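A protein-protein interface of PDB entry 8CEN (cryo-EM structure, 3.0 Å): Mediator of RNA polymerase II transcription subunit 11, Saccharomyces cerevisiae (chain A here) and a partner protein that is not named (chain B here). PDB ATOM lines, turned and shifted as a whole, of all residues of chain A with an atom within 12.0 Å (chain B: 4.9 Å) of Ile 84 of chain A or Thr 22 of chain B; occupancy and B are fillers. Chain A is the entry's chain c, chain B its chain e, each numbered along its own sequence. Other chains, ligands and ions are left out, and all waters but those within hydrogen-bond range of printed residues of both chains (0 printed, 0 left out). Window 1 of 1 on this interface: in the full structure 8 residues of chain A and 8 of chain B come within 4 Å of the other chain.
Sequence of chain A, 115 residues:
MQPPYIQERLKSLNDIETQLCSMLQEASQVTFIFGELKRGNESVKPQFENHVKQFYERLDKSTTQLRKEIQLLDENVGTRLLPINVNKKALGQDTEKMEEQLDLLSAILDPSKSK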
ATOM      1  N   LEU A  73     -22.181 -22.232  -4.930  1.00  0.00           N
ATOM      2  CA  LEU A  73     -22.353 -21.392  -6.113  1.00  0.00           C
ATOM      3  C   LEU A  73     -21.034 -20.766  -6.550  1.00  0.00           C
ATOM      4  O   LEU A  73     -20.736 -20.704  -7.749  1.00  0.00           O
ATOM      5  CB  LEU A  73     -23.392 -20.306  -5.831  1.00  0.00           C
ATOM      6  CG  LEU A  73     -23.646 -19.269  -6.927  1.00  0.00           C
ATOM      7  CD1 LEU A  73     -24.296 -19.910  -8.140  1.00  0.00           C
ATOM      8  CD2 LEU A  73     -24.499 -18.129  -6.397  1.00  0.00           C
ATOM      9  N   ASP A  74     -20.231 -20.300  -5.594  1.00  0.00           N
ATOM     10  CA  ASP A  74     -18.935 -19.727  -5.943  1.00  0.00           C
ATOM     11  C   ASP A  74     -17.921 -20.804  -6.315  1.00  0.00           C
ATOM     12  O   ASP A  74     -17.043 -20.563  -7.151  1.00  0.00           O
ATOM     13  CB  ASP A  74     -18.411 -18.874  -4.788  1.00  0.00           C
ATOM     14  CG  ASP A  74     -17.136 -18.136  -5.141  1.00  0.00           C
ATOM     15  OD1 ASP A  74     -17.213 -17.146  -5.900  1.00  0.00           O
ATOM     16  OD2 ASP A  74     -16.057 -18.544  -4.663  1.00  0.00           O
ATOM     17  N   GLU A  75     -18.025 -21.991  -5.710  1.00  0.00           N
ATOM     18  CA  GLU A  75     -17.075 -23.065  -5.982  1.00  0.00           C
ATOM     19  C   GLU A  75     -17.281 -23.650  -7.373  1.00  0.00           C
ATOM     20  O   GLU A  75     -16.309 -23.946  -8.079  1.00  0.00           O
ATOM     21  CB  GLU A  75     -17.208 -24.148  -4.909  1.00  0.00           C
ATOM     22  CG  GLU A  75     -16.600 -25.495  -5.268  1.00  0.00           C
ATOM     23  CD  GLU A  75     -16.816 -26.536  -4.187  1.00  0.00           C
ATOM     24  OE1 GLU A  75     -17.553 -26.245  -3.221  1.00  0.00           O
ATOM     25  OE2 GLU A  75     -16.251 -27.644  -4.303  1.00  0.00           O
ATOM     26  N   ASN A  76     -18.535 -23.797  -7.798  1.00  0.00           N
ATOM     27  CA  ASN A  76     -18.854 -24.399  -9.084  1.00  0.00           C
ATOM     28  C   ASN A  76     -18.809 -23.404 -10.237  1.00  0.00           C
ATOM     29  O   ASN A  76     -19.402 -23.666 -11.288  1.00  0.00           O
ATOM     30  CB  ASN A  76     -20.228 -25.070  -9.023  1.00  0.00           C
ATOM     31  CG  ASN A  76     -20.300 -26.148  -7.962  1.00  0.00           C
ATOM     32  OD1 ASN A  76     -21.383 -26.607  -7.603  1.00  0.00           O
ATOM     33  ND2 ASN A  76     -19.144 -26.556  -7.453  1.00  0.00           N
ATOM     34  N   VAL A  77     -18.110 -22.277 -10.069  1.00  0.00           N
ATOM     35  CA  VAL A  77     -17.986 -21.300 -11.143  1.00  0.00           C
ATOM     36  C   VAL A  77     -17.112 -21.823 -12.281  1.00  0.00           C
ATOM     37  O   VAL A  77     -17.170 -21.298 -13.399  1.00  0.00           O
ATOM     38  CB  VAL A  77     -17.448 -19.969 -10.571  1.00  0.00           C
ATOM     39  CG1 VAL A  77     -15.953 -20.062 -10.277  1.00  0.00           C
ATOM     40  CG2 VAL A  77     -17.767 -18.794 -11.493  1.00  0.00           C
ATOM     41  N   GLY A  78     -16.320 -22.867 -12.040  1.00  0.00           N
ATOM     42  CA  GLY A  78     -15.483 -23.424 -13.081  1.00  0.00           C
ATOM     43  C   GLY A  78     -15.881 -24.823 -13.501  1.00  0.00           C
ATOM     44  O   GLY A  78     -15.528 -25.273 -14.594  1.00  0.00           O
ATOM     45  N   THR A  79     -16.625 -25.523 -12.642  1.00  0.00           N
ATOM     46  CA  THR A  79     -16.966 -26.914 -12.919  1.00  0.00           C
ATOM     47  C   THR A  79     -18.164 -27.022 -13.855  1.00  0.00           C
ATOM     48  O   THR A  79     -18.147 -27.797 -14.816  1.00  0.00           O
ATOM     49  CB  THR A  79     -17.255 -27.656 -11.610  1.00  0.00           C
ATOM     50  OG1 THR A  79     -18.375 -27.053 -10.952  1.00  0.00           O
ATOM     51  CG2 THR A  79     -16.047 -27.605 -10.688  1.00  0.00           C
ATOM     52  N   ARG A  80     -19.224 -26.268 -13.570  1.00  0.00           N
ATOM     53  CA  ARG A  80     -20.458 -26.357 -14.334  1.00  0.00           C
ATOM     54  C   ARG A  80     -21.202 -25.033 -14.443  1.00  0.00           C
ATOM     55  O   ARG A  80     -22.390 -25.032 -14.782  1.00  0.00           O
ATOM     56  CB  ARG A  80     -21.351 -27.444 -13.733  1.00  0.00           C
ATOM     57  CG  ARG A  80     -21.887 -27.148 -12.346  1.00  0.00           C
ATOM     58  CD  ARG A  80     -22.634 -28.377 -11.885  1.00  0.00           C
ATOM     59  NE  ARG A  80     -21.656 -29.438 -11.684  1.00  0.00           N
ATOM     60  CZ  ARG A  80     -21.951 -30.702 -11.431  1.00  0.00           C
ATOM     61  NH1 ARG A  80     -23.202 -31.118 -11.373  1.00  0.00           N
ATOM     62  NH2 ARG A  80     -20.964 -31.577 -11.267  1.00  0.00           N
ATOM     63  N   LEU A  81     -20.538 -23.913 -14.171  1.00  0.00           N
ATOM     64  CA  LEU A  81     -21.075 -22.589 -14.437  1.00  0.00           C
ATOM     65  C   LEU A  81     -20.133 -21.834 -15.364  1.00  0.00           C
ATOM     66  O   LEU A  81     -18.946 -22.148 -15.465  1.00  0.00           O
ATOM     67  CB  LEU A  81     -21.287 -21.779 -13.148  1.00  0.00           C
ATOM     68  CG  LEU A  81     -22.596 -21.933 -12.372  1.00  0.00           C
ATOM     69  CD1 LEU A  81     -22.645 -23.236 -11.597  1.00  0.00           C
ATOM     70  CD2 LEU A  81     -22.773 -20.749 -11.438  1.00  0.00           C
ATOM     71  N   LEU A  82     -20.681 -20.844 -16.054  1.00  0.00           N
ATOM     72  CA  LEU A  82     -19.865 -20.016 -16.931  1.00  0.00           C
ATOM     73  C   LEU A  82     -18.980 -19.097 -16.095  1.00  0.00           C
ATOM     74  O   LEU A  82     -19.487 -18.397 -15.210  1.00  0.00           O
ATOM     75  CB  LEU A  82     -20.748 -19.194 -17.866  1.00  0.00           C
ATOM     76  CG  LEU A  82     -21.591 -19.966 -18.882  1.00  0.00           C
ATOM     77  CD1 LEU A  82     -22.644 -19.064 -19.521  1.00  0.00           C
ATOM     78  CD2 LEU A  82     -20.703 -20.608 -19.940  1.00  0.00           C
ATOM     79  N   PRO A  83     -17.665 -19.075 -16.331  1.00  0.00           N
ATOM     80  CA  PRO A  83     -16.800 -18.157 -15.573  1.00  0.00           C
ATOM     81  C   PRO A  83     -17.000 -16.695 -15.936  1.00  0.00           C
ATOM     82  O   PRO A  83     -16.547 -15.820 -15.189  1.00  0.00           O
ATOM     83  CB  PRO A  83     -15.387 -18.635 -15.931  1.00  0.00           C
ATOM     84  CG  PRO A  83     -15.541 -19.242 -17.287  1.00  0.00           C
ATOM     85  CD  PRO A  83     -16.911 -19.864 -17.320  1.00  0.00           C
ATOM     86  N   ILE A  84     -17.661 -16.406 -17.058  1.00  0.00           N
ATOM     87  CA  ILE A  84     -17.989 -15.051 -17.472  1.00  0.00           C
ATOM     88  C   ILE A  84     -19.502 -14.957 -17.632  1.00  0.00           C
ATOM     89  O   ILE A  84     -20.214 -15.961 -17.622  1.00  0.00           O
ATOM     90  CB  ILE A  84     -17.283 -14.654 -18.784  1.00  0.00           C
ATOM     91  CG1 ILE A  84     -17.740 -15.569 -19.919  1.00  0.00           C
ATOM     92  CG2 ILE A  84     -15.773 -14.709 -18.618  1.00  0.00           C
ATOM     93  CD1 ILE A  84     -17.291 -15.126 -21.286  1.00  0.00           C
ATOM     94  N   ASN A  85     -19.990 -13.729 -17.777  1.00  0.00           N
ATOM     95  CA  ASN A  85     -21.416 -13.470 -17.965  1.00  0.00           C
ATOM     96  C   ASN A  85     -21.662 -13.212 -19.447  1.00  0.00           C
ATOM     97  O   ASN A  85     -21.353 -12.134 -19.962  1.00  0.00           O
ATOM     98  CB  ASN A  85     -21.874 -12.296 -17.106  1.00  0.00           C
ATOM     99  CG  ASN A  85     -21.847 -12.613 -15.623  1.00  0.00           C
ATOM    100  OD1 ASN A  85     -21.279 -13.621 -15.200  1.00  0.00           O
ATOM    101  ND2 ASN A  85     -22.463 -11.749 -14.823  1.00  0.00           N
ATOM    102  N   VAL A  86     -22.219 -14.206 -20.132  1.00  0.00           N
ATOM    103  CA  VAL A  86     -22.499 -14.105 -21.561  1.00  0.00           C
ATOM    104  C   VAL A  86     -23.750 -14.921 -21.863  1.00  0.00           C
ATOM    105  O   VAL A  86     -24.006 -15.950 -21.230  1.00  0.00           O
ATOM    106  CB  VAL A  86     -21.275 -14.548 -22.400  1.00  0.00           C
ATOM    107  CG1 VAL A  86     -20.959 -16.030 -22.200  1.00  0.00           C
ATOM    108  CG2 VAL A  86     -21.479 -14.233 -23.876  1.00  0.00           C
ATOM    109  N   ASN A  87     -24.562 -14.426 -22.796  1.00  0.00           N
ATOM    110  CA  ASN A  87     -25.730 -15.171 -23.243  1.00  0.00           C
ATOM    111  C   ASN A  87     -25.305 -16.357 -24.098  1.00  0.00           C
ATOM    112  O   ASN A  87     -24.410 -16.248 -24.942  1.00  0.00           O
ATOM    113  CB  ASN A  87     -26.674 -14.266 -24.037  1.00  0.00           C
ATOM    114  CG  ASN A  87     -25.948 -13.433 -25.074  1.00  0.00           C
ATOM    115  OD1 ASN A  87     -24.970 -12.752 -24.766  1.00  0.00           O
ATOM    116  ND2 ASN A  87     -26.422 -13.486 -26.314  1.00  0.00           N
ATOM    117  N   LYS A  88     -25.956 -17.494 -23.881  1.00  0.00           N
ATOM    118  CA  LYS A  88     -25.614 -18.710 -24.598  1.00  0.00           C
ATOM    119  C   LYS A  88     -26.225 -18.701 -25.999  1.00  0.00           C
ATOM    120  O   LYS A  88     -26.974 -17.799 -26.380  1.00  0.00           O
ATOM    121  CB  LYS A  88     -26.080 -19.939 -23.818  1.00  0.00           C
ATOM    122  CG  LYS A  88     -25.349 -20.156 -22.505  1.00  0.00           C
ATOM    123  CD  LYS A  88     -25.746 -21.478 -21.865  1.00  0.00           C
ATOM    124  CE  LYS A  88     -27.144 -21.410 -21.272  1.00  0.00           C
ATOM    125  NZ  LYS A  88     -27.506 -22.660 -20.546  1.00  0.00           N
ATOM    126  N   LYS A  89     -25.890 -19.731 -26.772  1.00  0.00           N
ATOM    127  CA  LYS A  89     -26.360 -19.879 -28.141  1.00  0.00           C
ATOM    128  C   LYS A  89     -27.162 -21.165 -28.282  1.00  0.00           C
ATOM    129  O   LYS A  89     -26.902 -22.158 -27.597  1.00  0.00           O
ATOM    130  CB  LYS A  89     -25.189 -19.892 -29.131  1.00  0.00           C
ATOM    131  CG  LYS A  89     -24.364 -18.617 -29.148  1.00  0.00           C
ATOM    132  CD  LYS A  89     -25.167 -17.450 -29.693  1.00  0.00           C
ATOM    133  CE  LYS A  89     -24.319 -16.192 -29.784  1.00  0.00           C
ATOM    134  NZ  LYS A  89     -25.108 -15.031 -30.278  1.00  0.00           N
ATOM    135  N   ALA A  90     -28.144 -21.137 -29.179  1.00  0.00           N
ATOM    136  CA  ALA A  90     -28.954 -22.311 -29.484  1.00  0.00           C
ATOM    137  C   ALA A  90     -28.290 -23.090 -30.612  1.00  0.00           C
ATOM    138  O   ALA A  90     -28.165 -22.584 -31.733  1.00  0.00           O
ATOM    139  CB  ALA A  90     -30.376 -21.905 -29.869  1.00  0.00           C
ATOM    140  N   LEU A  91     -27.871 -24.318 -30.318  1.00  0.00           N
ATOM    141  CA  LEU A  91     -27.091 -25.120 -31.247  1.00  0.00           C
ATOM    142  C   LEU A  91     -27.755 -26.473 -31.472  1.00  0.00           C
ATOM    143  O   LEU A  91     -28.428 -27.008 -30.586  1.00  0.00           O
ATOM    144  CB  LEU A  91     -25.661 -25.329 -30.725  1.00  0.00           C
ATOM    145  CG  LEU A  91     -24.874 -24.082 -30.311  1.00  0.00           C
ATOM    146  CD1 LEU A  91     -23.542 -24.470 -29.688  1.00  0.00           C
ATOM    147  CD2 LEU A  91     -24.661 -23.149 -31.495  1.00  0.00           C
ATOM    148  N   LEU B  18     -12.928 -26.257 -19.881  1.00  0.00           N
ATOM    149  CA  LEU B  18     -13.742 -25.122 -19.462  1.00  0.00           C
ATOM    150  C   LEU B  18     -13.634 -23.968 -20.451  1.00  0.00           C
ATOM    151  O   LEU B  18     -14.649 -23.351 -20.803  1.00  0.00           O
ATOM    152  CB  LEU B  18     -13.338 -24.676 -18.057  1.00  0.00           C
ATOM    153  CG  LEU B  18     -13.968 -23.378 -17.549  1.00  0.00           C
ATOM    154  CD1 LEU B  18     -15.473 -23.533 -17.407  1.00  0.00           C
ATOM    155  CD2 LEU B  18     -13.347 -22.974 -16.223  1.00  0.00           C
ATOM    156  N   LEU B  19     -12.420 -23.677 -20.931  1.00  0.00           N
ATOM    157  CA  LEU B  19     -12.268 -22.631 -21.938  1.00  0.00           C
ATOM    158  C   LEU B  19     -12.921 -23.034 -23.256  1.00  0.00           C
ATOM    159  O   LEU B  19     -13.497 -22.187 -23.946  1.00  0.00           O
ATOM    160  CB  LEU B  19     -10.791 -22.288 -22.149  1.00  0.00           C
ATOM    161  CG  LEU B  19     -10.562 -21.143 -23.147  1.00  0.00           C
ATOM    162  CD1 LEU B  19     -11.191 -19.855 -22.639  1.00  0.00           C
ATOM    163  CD2 LEU B  19      -9.102 -20.917 -23.481  1.00  0.00           C
ATOM    164  N   ILE B  20     -12.857 -24.322 -23.614  1.00  0.00           N
ATOM    165  CA  ILE B  20     -13.500 -24.795 -24.841  1.00  0.00           C
ATOM    166  C   ILE B  20     -15.008 -24.576 -24.775  1.00  0.00           C
ATOM    167  O   ILE B  20     -15.618 -24.052 -25.716  1.00  0.00           O
ATOM    168  CB  ILE B  20     -13.152 -26.273 -25.099  1.00  0.00           C
ATOM    169  CG1 ILE B  20     -11.723 -26.403 -25.632  1.00  0.00           C
ATOM    170  CG2 ILE B  20     -14.131 -26.906 -26.079  1.00  0.00           C
ATOM    171  CD1 ILE B  20     -11.451 -25.561 -26.851  1.00  0.00           C
ATOM    172  N   SER B  21     -15.623 -24.941 -23.645  1.00  0.00           N
ATOM    173  CA  SER B  21     -17.060 -24.728 -23.477  1.00  0.00           C
ATOM    174  C   SER B  21     -17.410 -23.242 -23.460  1.00  0.00           C
ATOM    175  O   SER B  21     -18.411 -22.826 -24.061  1.00  0.00           O
ATOM    176  CB  SER B  21     -17.544 -25.408 -22.198  1.00  0.00           C
ATOM    177  OG  SER B  21     -16.806 -24.962 -21.074  1.00  0.00           O
ATOM    178  N   THR B  22     -16.589 -22.427 -22.788  1.00  0.00           N
ATOM    179  CA  THR B  22     -16.850 -20.991 -22.708  1.00  0.00           C
ATOM    180  C   THR B  22     -16.780 -20.335 -24.084  1.00  0.00           C
ATOM    181  O   THR B  22     -17.654 -19.543 -24.452  1.00  0.00           O
ATOM    182  CB  THR B  22     -15.855 -20.337 -21.748  1.00  0.00           C
ATOM    183  OG1 THR B  22     -15.910 -21.000 -20.479  1.00  0.00           O
ATOM    184  CG2 THR B  22     -16.185 -18.866 -21.554  1.00  0.00           C
ATOM    185  N   LEU B  23     -15.760 -20.678 -24.872  1.00  0.00           N
ATOM    186  CA  LEU B  23     -15.635 -20.114 -26.211  1.00  0.00           C
ATOM    187  C   LEU B  23     -16.685 -20.669 -27.163  1.00  0.00           C
ATOM    188  O   LEU B  23     -17.081 -19.979 -28.107  1.00  0.00           O
ATOM    189  CB  LEU B  23     -14.233 -20.365 -26.753  1.00  0.00           C
ATOM    190  CG  LEU B  23     -13.135 -19.691 -25.934  1.00  0.00           C
ATOM    191  CD1 LEU B  23     -11.789 -20.079 -26.473  1.00  0.00           C
ATOM    192  CD2 LEU B  23     -13.307 -18.182 -25.946  1.00  0.00           C
ATOM    193  N   THR B  24     -17.148 -21.902 -26.932  1.00  0.00           N
ATOM    194  CA  THR B  24     -18.283 -22.413 -27.692  1.00  0.00           C
ATOM    195  C   THR B  24     -19.534 -21.588 -27.418  1.00  0.00           C
ATOM    196  O   THR B  24     -20.290 -21.272 -28.341  1.00  0.00           O
ATOM    197  CB  THR B  24     -18.524 -23.885 -27.354  1.00  0.00           C
ATOM    198  OG1 THR B  24     -17.279 -24.595 -27.389  1.00  0.00           O
ATOM    199  CG2 THR B  24     -19.481 -24.511 -28.353  1.00  0.00           C
ATOM    200  N   THR B  25     -19.755 -21.216 -26.154  1.00  0.00           N
ATOM    201  CA  THR B  25     -20.876 -20.337 -25.829  1.00  0.00           C
ATOM    202  C   THR B  25     -20.697 -18.947 -26.436  1.00  0.00           C
ATOM    203  O   THR B  25     -21.673 -18.322 -26.868  1.00  0.00           O
ATOM    204  CB  THR B  25     -21.057 -20.231 -24.315  1.00  0.00           C
ATOM    205  OG1 THR B  25     -19.849 -19.744 -23.719  1.00  0.00           O
ATOM    206  CG2 THR B  25     -21.410 -21.580 -23.726  1.00  0.00           C
ATOM    207  N   ILE B  26     -19.462 -18.441 -26.456  1.00  0.00           N
ATOM    208  CA  ILE B  26     -19.206 -17.108 -27.001  1.00  0.00           C
ATOM    209  C   ILE B  26     -19.458 -17.074 -28.506  1.00  0.00           C
ATOM    210  O   ILE B  26     -20.163 -16.194 -29.014  1.00  0.00           O
ATOM    211  CB  ILE B  26     -17.775 -16.651 -26.663  1.00  0.00           C
ATOM    212  CG1 ILE B  26     -17.618 -16.424 -25.159  1.00  0.00           C
ATOM    213  CG2 ILE B  26     -17.399 -15.406 -27.458  1.00  0.00           C
ATOM    214  CD1 ILE B  26     -16.231 -15.993 -24.754  1.00  0.00           C
ATOM    215  N   GLU B 281     -14.980  -9.206 -22.736  1.00  0.00           N
ATOM    216  CA  GLU B 281     -15.831 -10.369 -22.522  1.00  0.00           C
ATOM    217  C   GLU B 281     -15.092 -11.472 -21.768  1.00  0.00           C
ATOM    218  O   GLU B 281     -15.714 -12.241 -21.029  1.00  0.00           O
ATOM    219  CB  GLU B 281     -16.355 -10.867 -23.872  1.00  0.00           C
ATOM    220  CG  GLU B 281     -17.328 -12.026 -23.810  1.00  0.00           C
ATOM    221  CD  GLU B 281     -17.836 -12.420 -25.181  1.00  0.00           C
ATOM    222  OE1 GLU B 281     -17.410 -11.802 -26.180  1.00  0.00           O
ATOM    223  OE2 GLU B 281     -18.675 -13.336 -25.259  1.00  0.00           O
ATOM    224  N   LEU B 282     -13.770 -11.548 -21.919  1.00  0.00           N
ATOM    225  CA  LEU B 282     -12.973 -12.588 -21.279  1.00  0.00           C
ATOM    226  C   LEU B 282     -12.345 -12.177 -19.950  1.00  0.00           C
ATOM    227  O   LEU B 282     -11.656 -13.002 -19.343  1.00  0.00           O
ATOM    228  CB  LEU B 282     -11.869 -13.064 -22.230  1.00  0.00           C
ATOM    229  CG  LEU B 282     -12.288 -13.914 -23.430  1.00  0.00           C
ATOM    230  CD1 LEU B 282     -11.069 -14.385 -24.201  1.00  0.00           C
ATOM    231  CD2 LEU B 282     -13.104 -15.103 -22.960  1.00  0.00           C
ATOM    232  N   GLN B 283     -12.542 -10.941 -19.487  1.00  0.00           N
ATOM    233  CA  GLN B 283     -11.989 -10.548 -18.192  1.00  0.00           C
ATOM    234  C   GLN B 283     -12.634 -11.323 -17.047  1.00  0.00           C
ATOM    235  O   GLN B 283     -13.791 -11.747 -17.121  1.00  0.00           O
ATOM    236  CB  GLN B 283     -12.149  -9.045 -17.942  1.00  0.00           C
ATOM    237  CG  GLN B 283     -11.333  -8.154 -18.857  1.00  0.00           C
ATOM    238  CD  GLN B 283     -11.539  -6.677 -18.587  1.00  0.00           C
ATOM    239  OE1 GLN B 283     -12.353  -6.295 -17.746  1.00  0.00           O
ATOM    240  NE2 GLN B 283     -10.798  -5.837 -19.300  1.00  0.00           N
ATOM    241  N   TYR B 285     -11.866 -14.352 -16.067  1.00  0.00           N
ATOM    242  CA  TYR B 285     -11.412 -15.726 -16.252  1.00  0.00           C
ATOM    243  C   TYR B 285      -9.952 -15.773 -16.697  1.00  0.00           C
ATOM    244  O   TYR B 285      -9.099 -16.328 -15.996  1.00  0.00           O
ATOM    245  CB  TYR B 285     -12.320 -16.431 -17.268  1.00  0.00           C
ATOM    246  CG  TYR B 285     -11.976 -17.879 -17.552  1.00  0.00           C
ATOM    247  CD1 TYR B 285     -11.511 -18.720 -16.546  1.00  0.00           C
ATOM    248  CD2 TYR B 285     -12.122 -18.404 -18.829  1.00  0.00           C
ATOM    249  CE1 TYR B 285     -11.197 -20.041 -16.810  1.00  0.00           C
ATOM    250  CE2 TYR B 285     -11.814 -19.722 -19.099  1.00  0.00           C
ATOM    251  CZ  TYR B 285     -11.351 -20.535 -18.088  1.00  0.00           C
ATOM    252  OH  TYR B 285     -11.041 -21.849 -18.358  1.00  0.00           O
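The side-chain hydroxyl (OG) of Ser 21 of chain B sits at hydrogen-bond distance from the backbone carbonyl oxygen (O) of Leu 18 of chain B (2.7 Å). N of Leu 19 of chain B lies within hydrogen-bond range of OH of Tyr 285 of chain B (3.4 Å). OG1 of Thr 25 of chain B lies close to O of Ser 21 of chain B (3.4 Å). The side-chain hydroxyl of Thr 22 of chain B is in hydrogen-bond range of the backbone carbonyl oxygen of Leu 18 of chain B, at 2.7 Å.
Among the printed residues, merely in contact across the chains: Gly 78 of chain A with Leu 18 of chain B, Leu 82 of chain A with Thr 25 of chain B, Pro 83 of chain A with Leu 18 of chain B, Pro 83 of chain A with Thr 22 of chain B, Pro 83 of chain A with Tyr 285 of chain B, Ile 84 of chain A with Thr 22 of chain B, Ile 84 of chain A with Ile 26 of chain B, Ile 84 of chain A with Glu 281 of chain B, Ile 84 of chain A with Gln 283 of chain B, Val 86 of chain A with Glu 281 of chain B, Asn 87 of chain A with Thr 25 of chain B and Lys 89 of chain A with Thr 25 of chain B.
Leu 73 of chain A touches none of the printed residues of chain B. Printed residues of chain B within 4 Å of Gly 78 of chain A: Leu 18. Of chain B, only Thr 22 (3.9 Å), Ile 26 (3.7 Å), Glu 281 (3.3 Å) and Gln 283 (3.9 Å) come within 4 Å of Ile 84 of chain A. Of the printed residues of chain B, Val 86 of chain A touches Glu 281. Of the printed residues of chain B, Asn 87 of chain A touches Thr 25 (3.9 Å). Of chain A, only Gly 78 (3.3 Å) and Pro 83 (3.9 Å) come within 4 Å of Leu 18 of chain B. No residue of chain A comes within 4 Å of Ser 21 of chain B. Of chain A, only Pro 83 and Ile 84 come within 4 Å of Thr 22 of chain B. No residue of chain A comes within 4 Å of Thr 24 of chain B. Thr 25 of chain B touches just these residues of chain A: Leu 82, Asn 87 and Lys 89. Of chain A, only Ile 84 comes within 4 Å of Ile 26 of chain B. Of the printed residues of chain A, Gln 283 of chain B touches Ile 84 (3.9 Å). Of chain A, only Pro 83 (3.8 Å) comes within 4 Å of Tyr 285 of chain B. The nearest residue of chain B that does not touch Ile 84 of chain A is Tyr 285 of chain B (4.1 Å). The nearest residue of chain A that does not touch Thr 22 of chain B is Leu 82 of chain A (4.8 Å).
Printed residues of chain A that touch a printed residue of chain B: Gly 78, Leu 82, Pro 83, Ile 84, Val 86, Asn 87 and Lys 89. Among the printed residues, 12 pairs touch across the chains.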
